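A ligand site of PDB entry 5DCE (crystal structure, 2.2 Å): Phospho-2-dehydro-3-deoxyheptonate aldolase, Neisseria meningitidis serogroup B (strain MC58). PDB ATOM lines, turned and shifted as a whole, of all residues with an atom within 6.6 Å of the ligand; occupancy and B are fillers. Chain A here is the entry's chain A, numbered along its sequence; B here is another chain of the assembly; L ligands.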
ATOM      1  N   ARG A  42      -7.467  32.512 -32.385  1.00  0.00           N
ATOM      2  CA  ARG A  42      -8.438  31.589 -32.942  1.00  0.00           C
ATOM      3  C   ARG A  42      -9.580  32.350 -33.602  1.00  0.00           C
ATOM      4  O   ARG A  42      -9.965  32.020 -34.727  1.00  0.00           O
ATOM      5  CB  ARG A  42      -8.965  30.628 -31.889  1.00  0.00           C
ATOM      6  CG  ARG A  42      -7.973  29.542 -31.528  1.00  0.00           C
ATOM      7  CD  ARG A  42      -8.476  28.817 -30.295  1.00  0.00           C
ATOM      8  NE  ARG A  42      -7.621  27.728 -29.832  1.00  0.00           N
ATOM      9  CZ  ARG A  42      -7.892  27.005 -28.763  1.00  0.00           C
ATOM     10  NH1 ARG A  42      -8.990  27.249 -28.051  1.00  0.00           N
ATOM     11  NH2 ARG A  42      -7.067  26.052 -28.367  1.00  0.00           N
ATOM     12  N   PHE A 146      -2.247  17.485 -35.269  1.00  0.00           N
ATOM     13  CA  PHE A 146      -2.714  16.451 -34.377  1.00  0.00           C
ATOM     14  C   PHE A 146      -2.796  15.104 -35.111  1.00  0.00           C
ATOM     15  O   PHE A 146      -3.620  14.927 -36.016  1.00  0.00           O
ATOM     16  CB  PHE A 146      -4.062  16.838 -33.844  1.00  0.00           C
ATOM     17  CG  PHE A 146      -4.066  18.124 -33.075  1.00  0.00           C
ATOM     18  CD1 PHE A 146      -3.542  18.180 -31.794  1.00  0.00           C
ATOM     19  CD2 PHE A 146      -4.605  19.261 -33.629  1.00  0.00           C
ATOM     20  CE1 PHE A 146      -3.549  19.341 -31.083  1.00  0.00           C
ATOM     21  CE2 PHE A 146      -4.622  20.433 -32.920  1.00  0.00           C
ATOM     22  CZ  PHE A 146      -4.095  20.472 -31.640  1.00  0.00           C
ATOM     23  N   MET A 149      -5.657  10.753 -31.216  1.00  0.00           N
ATOM     24  CA  MET A 149      -6.789  11.232 -30.503  1.00  0.00           C
ATOM     25  C   MET A 149      -6.502  11.519 -29.055  1.00  0.00           C
ATOM     26  O   MET A 149      -7.406  11.960 -28.364  1.00  0.00           O
ATOM     27  CB  MET A 149      -7.899  10.162 -30.524  1.00  0.00           C
ATOM     28  CG  MET A 149      -8.228   9.588 -31.868  1.00  0.00           C
ATOM     29  SD  MET A 149      -8.541  10.889 -33.042  1.00  0.00           S
ATOM     30  CE  MET A 149      -7.368  10.331 -34.262  1.00  0.00           C
ATOM     31  N   ILE A 150      -5.295  11.236 -28.582  1.00  0.00           N
ATOM     32  CA  ILE A 150      -4.981  11.353 -27.161  1.00  0.00           C
ATOM     33  C   ILE A 150      -4.056  12.531 -26.809  1.00  0.00           C
ATOM     34  O   ILE A 150      -4.371  13.318 -25.938  1.00  0.00           O
ATOM     35  CB  ILE A 150      -4.459  10.020 -26.677  1.00  0.00           C
ATOM     36  CG1 ILE A 150      -5.613   9.007 -26.756  1.00  0.00           C
ATOM     37  CG2 ILE A 150      -3.949  10.111 -25.256  1.00  0.00           C
ATOM     38  CD1 ILE A 150      -5.298   7.638 -26.238  1.00  0.00           C
ATOM     39  N   PRO A 152      -3.748  15.459 -28.014  1.00  0.00           N
ATOM     40  CA  PRO A 152      -4.351  16.779 -27.916  1.00  0.00           C
ATOM     41  C   PRO A 152      -4.797  17.224 -26.536  1.00  0.00           C
ATOM     42  O   PRO A 152      -4.825  18.425 -26.240  1.00  0.00           O
ATOM     43  CB  PRO A 152      -5.593  16.673 -28.797  1.00  0.00           C
ATOM     44  CG  PRO A 152      -5.308  15.591 -29.761  1.00  0.00           C
ATOM     45  CD  PRO A 152      -4.397  14.632 -29.054  1.00  0.00           C
ATOM     46  N   GLN A 153      -5.208  16.282 -25.685  1.00  0.00           N
ATOM     47  CA  GLN A 153      -5.611  16.648 -24.332  1.00  0.00           C
ATOM     48  C   GLN A 153      -4.439  17.263 -23.510  1.00  0.00           C
ATOM     49  O   GLN A 153      -4.661  17.941 -22.507  1.00  0.00           O
ATOM     50  CB  GLN A 153      -6.197  15.430 -23.612  1.00  0.00           C
ATOM     51  CG  GLN A 153      -7.575  15.008 -24.107  1.00  0.00           C
ATOM     52  CD  GLN A 153      -8.682  15.887 -23.549  1.00  0.00           C
ATOM     53  OE1 GLN A 153      -8.816  17.055 -23.936  1.00  0.00           O
ATOM     54  NE2 GLN A 153      -9.469  15.363 -22.623  1.00  0.00           N
ATOM     55  N   ALA A 156      -3.732  21.070 -26.387  1.00  0.00           N
ATOM     56  CA  ALA A 156      -4.579  21.711 -27.415  1.00  0.00           C
ATOM     57  C   ALA A 156      -5.036  23.090 -26.989  1.00  0.00           C
ATOM     58  O   ALA A 156      -5.266  24.002 -27.800  1.00  0.00           O
ATOM     59  CB  ALA A 156      -5.769  20.834 -27.732  1.00  0.00           C
ATOM     60  N   ASP A 157      -5.140  23.248 -25.687  1.00  0.00           N
ATOM     61  CA  ASP A 157      -5.456  24.542 -25.128  1.00  0.00           C
ATOM     62  C   ASP A 157      -4.431  25.622 -25.469  1.00  0.00           C
ATOM     63  O   ASP A 157      -4.726  26.799 -25.346  1.00  0.00           O
ATOM     64  CB  ASP A 157      -5.610  24.420 -23.605  1.00  0.00           C
ATOM     65  CG  ASP A 157      -4.315  23.980 -22.904  1.00  0.00           C
ATOM     66  OD1 ASP A 157      -3.609  23.121 -23.431  1.00  0.00           O
ATOM     67  OD2 ASP A 157      -4.031  24.456 -21.798  1.00  0.00           O
ATOM     68  N   LEU A 177     -12.241  14.007 -34.489  1.00  0.00           N
ATOM     69  CA  LEU A 177     -11.357  14.791 -33.625  1.00  0.00           C
ATOM     70  C   LEU A 177     -11.461  16.285 -33.959  1.00  0.00           C
ATOM     71  O   LEU A 177     -11.667  17.111 -33.098  1.00  0.00           O
ATOM     72  CB  LEU A 177      -9.919  14.334 -33.778  1.00  0.00           C
ATOM     73  CG  LEU A 177      -8.861  15.273 -33.188  1.00  0.00           C
ATOM     74  CD1 LEU A 177      -9.020  15.344 -31.682  1.00  0.00           C
ATOM     75  CD2 LEU A 177      -7.469  14.807 -33.533  1.00  0.00           C
ATOM     76  N   GLY A 180     -14.268  18.407 -32.664  1.00  0.00           N
ATOM     77  CA  GLY A 180     -14.265  18.824 -31.273  1.00  0.00           C
ATOM     78  C   GLY A 180     -13.062  19.667 -30.868  1.00  0.00           C
ATOM     79  O   GLY A 180     -12.942  20.041 -29.715  1.00  0.00           O
ATOM     80  N   LEU A 181     -12.187  19.982 -31.808  1.00  0.00           N
ATOM     81  CA  LEU A 181     -11.019  20.821 -31.486  1.00  0.00           C
ATOM     82  C   LEU A 181     -11.425  22.278 -31.311  1.00  0.00           C
ATOM     83  O   LEU A 181     -12.242  22.821 -32.067  1.00  0.00           O
ATOM     84  CB  LEU A 181      -9.936  20.696 -32.565  1.00  0.00           C
ATOM     85  CG  LEU A 181      -9.083  19.437 -32.572  1.00  0.00           C
ATOM     86  CD1 LEU A 181      -8.212  19.424 -33.815  1.00  0.00           C
ATOM     87  CD2 LEU A 181      -8.232  19.371 -31.324  1.00  0.00           C
ATOM     88  N   SER A 182     -10.867  22.926 -30.301  1.00  0.00           N
ATOM     89  CA  SER A 182     -11.187  24.311 -30.029  1.00  0.00           C
ATOM     90  C   SER A 182     -10.650  25.319 -31.074  1.00  0.00           C
ATOM     91  O   SER A 182     -11.138  26.441 -31.165  1.00  0.00           O
ATOM     92  CB  SER A 182     -10.682  24.678 -28.638  1.00  0.00           C
ATOM     93  OG  SER A 182     -11.245  23.807 -27.673  1.00  0.00           O
ATOM     94  N   CYS A 183      -9.666  24.897 -31.874  1.00  0.00           N
ATOM     95  CA  CYS A 183      -9.019  25.789 -32.812  1.00  0.00           C
ATOM     96  C   CYS A 183      -9.540  25.531 -34.204  1.00  0.00           C
ATOM     97  O   CYS A 183     -10.029  24.442 -34.498  1.00  0.00           O
ATOM     98  CB  CYS A 183      -7.536  25.519 -32.793  1.00  0.00           C
ATOM     99  SG  CYS A 183      -7.167  23.777 -33.143  1.00  0.00           S
ATOM    100  N   PHE A 211     -16.949  10.476 -30.410  1.00  0.00           N
ATOM    101  CA  PHE A 211     -15.748   9.671 -30.543  1.00  0.00           C
ATOM    102  C   PHE A 211     -15.180   9.330 -29.184  1.00  0.00           C
ATOM    103  O   PHE A 211     -15.542   9.914 -28.178  1.00  0.00           O
ATOM    104  CB  PHE A 211     -14.720  10.278 -31.519  1.00  0.00           C
ATOM    105  CG  PHE A 211     -13.897  11.414 -30.949  1.00  0.00           C
ATOM    106  CD1 PHE A 211     -14.355  12.711 -30.991  1.00  0.00           C
ATOM    107  CD2 PHE A 211     -12.624  11.173 -30.453  1.00  0.00           C
ATOM    108  CE1 PHE A 211     -13.589  13.747 -30.508  1.00  0.00           C
ATOM    109  CE2 PHE A 211     -11.846  12.204 -29.953  1.00  0.00           C
ATOM    110  CZ  PHE A 211     -12.335  13.495 -29.974  1.00  0.00           C
ATOM    111  N   LEU A 212     -14.340   8.309 -29.182  1.00  0.00           N
ATOM    112  CA  LEU A 212     -13.861   7.728 -27.970  1.00  0.00           C
ATOM    113  C   LEU A 212     -12.495   8.327 -27.768  1.00  0.00           C
ATOM    114  O   LEU A 212     -11.691   8.429 -28.707  1.00  0.00           O
ATOM    115  CB  LEU A 212     -13.797   6.214 -28.077  1.00  0.00           C
ATOM    116  CG  LEU A 212     -15.115   5.461 -28.327  1.00  0.00           C
ATOM    117  CD1 LEU A 212     -14.915   3.974 -28.076  1.00  0.00           C
ATOM    118  CD2 LEU A 212     -16.249   5.965 -27.486  1.00  0.00           C
ATOM    119  N   SER A 213     -12.252   8.772 -26.551  1.00  0.00           N
ATOM    120  CA  SER A 213     -10.989   9.372 -26.229  1.00  0.00           C
ATOM    121  C   SER A 213     -10.766   9.285 -24.738  1.00  0.00           C
ATOM    122  O   SER A 213     -11.308   8.421 -24.070  1.00  0.00           O
ATOM    123  CB  SER A 213     -10.961  10.830 -26.709  1.00  0.00           C
ATOM    124  OG  SER A 213      -9.609  11.264 -26.809  1.00  0.00           O
ATOM    125  N   VAL A 214      -9.947  10.173 -24.220  1.00  0.00           N
ATOM    126  CA  VAL A 214      -9.520  10.088 -22.856  1.00  0.00           C
ATOM    127  C   VAL A 214      -9.894  11.391 -22.202  1.00  0.00           C
ATOM    128  O   VAL A 214      -9.749  12.450 -22.833  1.00  0.00           O
ATOM    129  CB  VAL A 214      -8.012   9.846 -22.863  1.00  0.00           C
ATOM    130  CG1 VAL A 214      -7.426  10.004 -21.509  1.00  0.00           C
ATOM    131  CG2 VAL A 214      -7.739   8.436 -23.365  1.00  0.00           C
ATOM    132  N   THR A 215     -10.405  11.331 -20.978  1.00  0.00           N
ATOM    133  CA  THR A 215     -10.620  12.557 -20.178  1.00  0.00           C
ATOM    134  C   THR A 215      -9.281  13.225 -19.776  1.00  0.00           C
ATOM    135  O   THR A 215      -8.228  12.654 -19.946  1.00  0.00           O
ATOM    136  CB  THR A 215     -11.367  12.279 -18.881  1.00  0.00           C
ATOM    137  OG1 THR A 215     -10.532  11.491 -18.021  1.00  0.00           O
ATOM    138  CG2 THR A 215     -12.692  11.562 -19.166  1.00  0.00           C
ATOM    139  N   LYS A 216      -9.338  14.433 -19.236  1.00  0.00           N
ATOM    140  CA  LYS A 216      -8.119  15.085 -18.737  1.00  0.00           C
ATOM    141  C   LYS A 216      -7.498  14.234 -17.648  1.00  0.00           C
ATOM    142  O   LYS A 216      -6.310  14.289 -17.430  1.00  0.00           O
ATOM    143  CB  LYS A 216      -8.428  16.480 -18.180  1.00  0.00           C
ATOM    144  CG  LYS A 216      -8.870  17.496 -19.215  1.00  0.00           C
ATOM    145  CD  LYS A 216      -7.768  17.748 -20.224  1.00  0.00           C
ATOM    146  CE  LYS A 216      -7.967  19.067 -20.959  1.00  0.00           C
ATOM    147  NZ  LYS A 216      -9.063  18.960 -21.962  1.00  0.00           N
ATOM    148  N   ALA A 221     -13.432   7.806 -22.359  1.00  0.00           N
ATOM    149  CA  ALA A 221     -14.719   8.416 -22.271  1.00  0.00           C
ATOM    150  C   ALA A 221     -15.290   8.624 -23.669  1.00  0.00           C
ATOM    151  O   ALA A 221     -14.606   8.451 -24.664  1.00  0.00           O
ATOM    152  CB  ALA A 221     -14.609   9.730 -21.534  1.00  0.00           C
ATOM    153  N   VAL A 223     -16.697  11.319 -26.135  1.00  0.00           N
ATOM    154  CA  VAL A 223     -16.743  12.744 -26.307  1.00  0.00           C
ATOM    155  C   VAL A 223     -17.793  13.080 -27.358  1.00  0.00           C
ATOM    156  O   VAL A 223     -17.739  12.605 -28.495  1.00  0.00           O
ATOM    157  CB  VAL A 223     -15.370  13.355 -26.632  1.00  0.00           C
ATOM    158  CG1 VAL A 223     -14.230  12.663 -25.876  1.00  0.00           C
ATOM    159  CG2 VAL A 223     -15.104  13.307 -28.106  1.00  0.00           C
ATOM    160  N   ASP B   8     -10.422  25.694 -23.692  1.00  0.00           N
ATOM    161  CA  ASP B   8     -10.464  24.217 -23.462  1.00  0.00           C
ATOM    162  C   ASP B   8     -11.891  23.639 -23.598  1.00  0.00           C
ATOM    163  O   ASP B   8     -12.809  24.035 -22.871  1.00  0.00           O
ATOM    164  CB  ASP B   8      -9.898  23.869 -22.082  1.00  0.00           C
ATOM    165  CG  ASP B   8      -9.757  22.371 -21.870  1.00  0.00           C
ATOM    166  OD1 ASP B   8      -9.337  21.685 -22.819  1.00  0.00           O
ATOM    167  OD2 ASP B   8     -10.086  21.877 -20.769  1.00  0.00           O
ATOM    168  N   ASP B   9     -12.056  22.687 -24.517  1.00  0.00           N
ATOM    169  CA  ASP B   9     -13.351  22.041 -24.757  1.00  0.00           C
ATOM    170  C   ASP B   9     -14.493  23.021 -25.134  1.00  0.00           C
ATOM    171  O   ASP B   9     -15.654  22.810 -24.779  1.00  0.00           O
ATOM    172  CB  ASP B   9     -13.755  21.184 -23.533  1.00  0.00           C
ATOM    173  CG  ASP B   9     -12.751  20.063 -23.231  1.00  0.00           C
ATOM    174  OD1 ASP B   9     -11.846  19.795 -24.051  1.00  0.00           O
ATOM    175  OD2 ASP B   9     -12.873  19.446 -22.146  1.00  0.00           O
ATOM    176  N   ILE B  10     -14.144  24.074 -25.872  1.00  0.00           N
ATOM    177  CA  ILE B  10     -15.124  25.027 -26.385  1.00  0.00           C
ATOM    178  C   ILE B  10     -16.149  24.321 -27.294  1.00  0.00           C
ATOM    179  O   ILE B  10     -17.341  24.549 -27.149  1.00  0.00           O
ATOM    180  CB  ILE B  10     -14.447  26.197 -27.151  1.00  0.00           C
ATOM    181  N   LYS B  11     -15.678  23.459 -28.204  1.00  0.00           N
ATOM    182  CA  LYS B  11     -16.563  22.740 -29.150  1.00  0.00           C
ATOM    183  C   LYS B  11     -16.921  21.305 -28.716  1.00  0.00           C
ATOM    184  O   LYS B  11     -17.217  20.450 -29.535  1.00  0.00           O
ATOM    185  CB  LYS B  11     -15.950  22.751 -30.558  1.00  0.00           C
ATOM    186  CG  LYS B  11     -15.732  24.152 -31.101  1.00  0.00           C
ATOM    187  CD  LYS B  11     -14.941  24.174 -32.407  1.00  0.00           C
ATOM    188  CE  LYS B  11     -14.172  25.497 -32.563  1.00  0.00           C
ATOM    189  NZ  LYS B  11     -13.190  25.495 -33.678  1.00  0.00           N
ATOM    190  N   ILE B  12     -16.902  21.052 -27.402  1.00  0.00           N
ATOM    191  CA  ILE B  12     -17.367  19.775 -26.855  1.00  0.00           C
ATOM    192  C   ILE B  12     -18.735  19.999 -26.205  1.00  0.00           C
ATOM    193  O   ILE B  12     -18.888  20.861 -25.347  1.00  0.00           O
ATOM    194  CB  ILE B  12     -16.380  19.243 -25.791  1.00  0.00           C
ATOM    195  CG1 ILE B  12     -14.981  19.061 -26.405  1.00  0.00           C
ATOM    196  CG2 ILE B  12     -16.875  17.940 -25.174  1.00  0.00           C
ATOM    197  CD1 ILE B  12     -14.913  18.144 -27.610  1.00  0.00           C
ATOM    198  N   VAL B  15     -18.969  15.073 -22.347  1.00  0.00           N
ATOM    199  CA  VAL B  15     -18.069  13.951 -22.141  1.00  0.00           C
ATOM    200  C   VAL B  15     -18.858  12.948 -21.306  1.00  0.00           C
ATOM    201  O   VAL B  15     -19.341  13.319 -20.240  1.00  0.00           O
ATOM    202  CB  VAL B  15     -16.800  14.386 -21.394  1.00  0.00           C
ATOM    203  CG1 VAL B  15     -15.957  13.184 -20.991  1.00  0.00           C
ATOM    204  CG2 VAL B  15     -15.999  15.358 -22.259  1.00  0.00           C
HETATM  205  N1  LIG L   1      -9.515  19.263 -25.426  1.00  0.00           N
HETATM  206  C1  LIG L   1      -9.669  19.440 -26.911  1.00  0.00           C
HETATM  207  C2  LIG L   1      -9.866  20.899 -27.253  1.00  0.00           C
HETATM  208  O1  LIG L   1      -9.543  21.300 -28.373  1.00  0.00           O
HETATM  209  C3  LIG L   1     -10.841  18.602 -27.484  1.00  0.00           C
HETATM  210  C4  LIG L   1     -10.638  17.152 -27.257  1.00  0.00           C
HETATM  211  C5  LIG L   1      -9.861  16.282 -27.980  1.00  0.00           C
HETATM  212  C6  LIG L   1     -11.159  16.411 -26.163  1.00  0.00           C
HETATM  213  N2  LIG L   1      -9.887  15.038 -27.395  1.00  0.00           N
HETATM  214  C7  LIG L   1     -10.688  15.094 -26.290  1.00  0.00           C
HETATM  215  C8  LIG L   1     -11.995  16.745 -25.089  1.00  0.00           C
HETATM  216  C9  LIG L   1     -11.019  14.117 -25.377  1.00  0.00           C
HETATM  217  C10 LIG L   1     -12.315  15.777 -24.186  1.00  0.00           C
HETATM  218  C11 LIG L   1     -11.827  14.463 -24.330  1.00  0.00           C
HETATM  219  O2  LIG L   1     -10.371  21.671 -26.443  1.00  0.00           O
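Ala 156 touches the ligand (CB to O1, 3.9 Å).
Leu 177 touches the ligand (CD1 to C5, 3.9 Å).
Gly 180 touches the ligand (O to C3, 3.4 Å).
Leu 181 touches the ligand.
Phe 211 touches the ligand.
OG of Ser 213 touches C9 of the ligand, 3.5 Å away.
Val 214 touches the ligand.
Lys 216 touches the ligand.
CG1 of Val 223 touches C11 of the ligand, at 3.4 Å.
Hydrophobic or aromatic side chains that line the ligand: Ala 156, Leu 177, Leu 181, Phe 211 and Val 223.
Within 4 Å of the ligand: Gln 153, Ala 156, Leu 177, Gly 180, Leu 181, Ser 182, Phe 211, Ser 213, Val 214, Lys 216, Val 223, Asp 8 of chain B and Asp 9 of chain B.
The nearest printed residue that does not touch the ligand is Ile 12 of chain B (4.001 Å).
The backbone NH (N) of Ser 182 lies within hydrogen-bond range of an oxygen (O1) of the ligand, 2.8 Å away.
The side-chain hydroxyl (OG) of Ser 182 sits at hydrogen-bond distance from an oxygen (O2) of the ligand (2.6 Å).
N of Asp 9 of chain B lies within hydrogen-bond range of O2 of the ligand, at 2.8 Å.
A nitrogen (N1) of the ligand is in salt-bridge range of the side-chain carboxylate (OD1) of Asp 9 of chain B, at 2.8 Å.
N1 of the ligand sits at hydrogen-bond distance from OE1 of Gln 153, 2.8 Å away.
The side-chain carboxylate (OD1) of Asp 8 of chain B is in salt-bridge range of a nitrogen (N1) of the ligand (3.6 Å).
OG of Ser 182 sits at hydrogen-bond distance from N of Ile 10 of chain B (3.4 Å).
The side-chain amino group (NZ) of Lys 11 of chain B sits at hydrogen-bond distance from the backbone carbonyl oxygen (O) of Ser 182.
The side-chain carboxylate (OD1) of Asp 9 of chain B is in salt-bridge range of the side-chain amino group (NZ) of Lys 216 (3.6 Å).
The backbone carbonyl oxygen (O) of Leu 181 sits close to the side-chain amino group (NZ) of Lys 11 of chain B (3.3 Å).
The backbone carbonyl oxygen of Met 149 is in hydrogen-bond range of the side-chain hydroxyl of Ser 213 (2.8 Å).
N of Ala 221 lies within hydrogen-bond range of O of Ser 213.
NZ of Lys 216 lies within salt-bridge range of OD1 of Asp 8 of chain B, 2.9 Å away.
The guanidinium group (NH2) of Arg 42 lies within hydrogen-bond range of the backbone carbonyl oxygen (O) of Ala 156.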
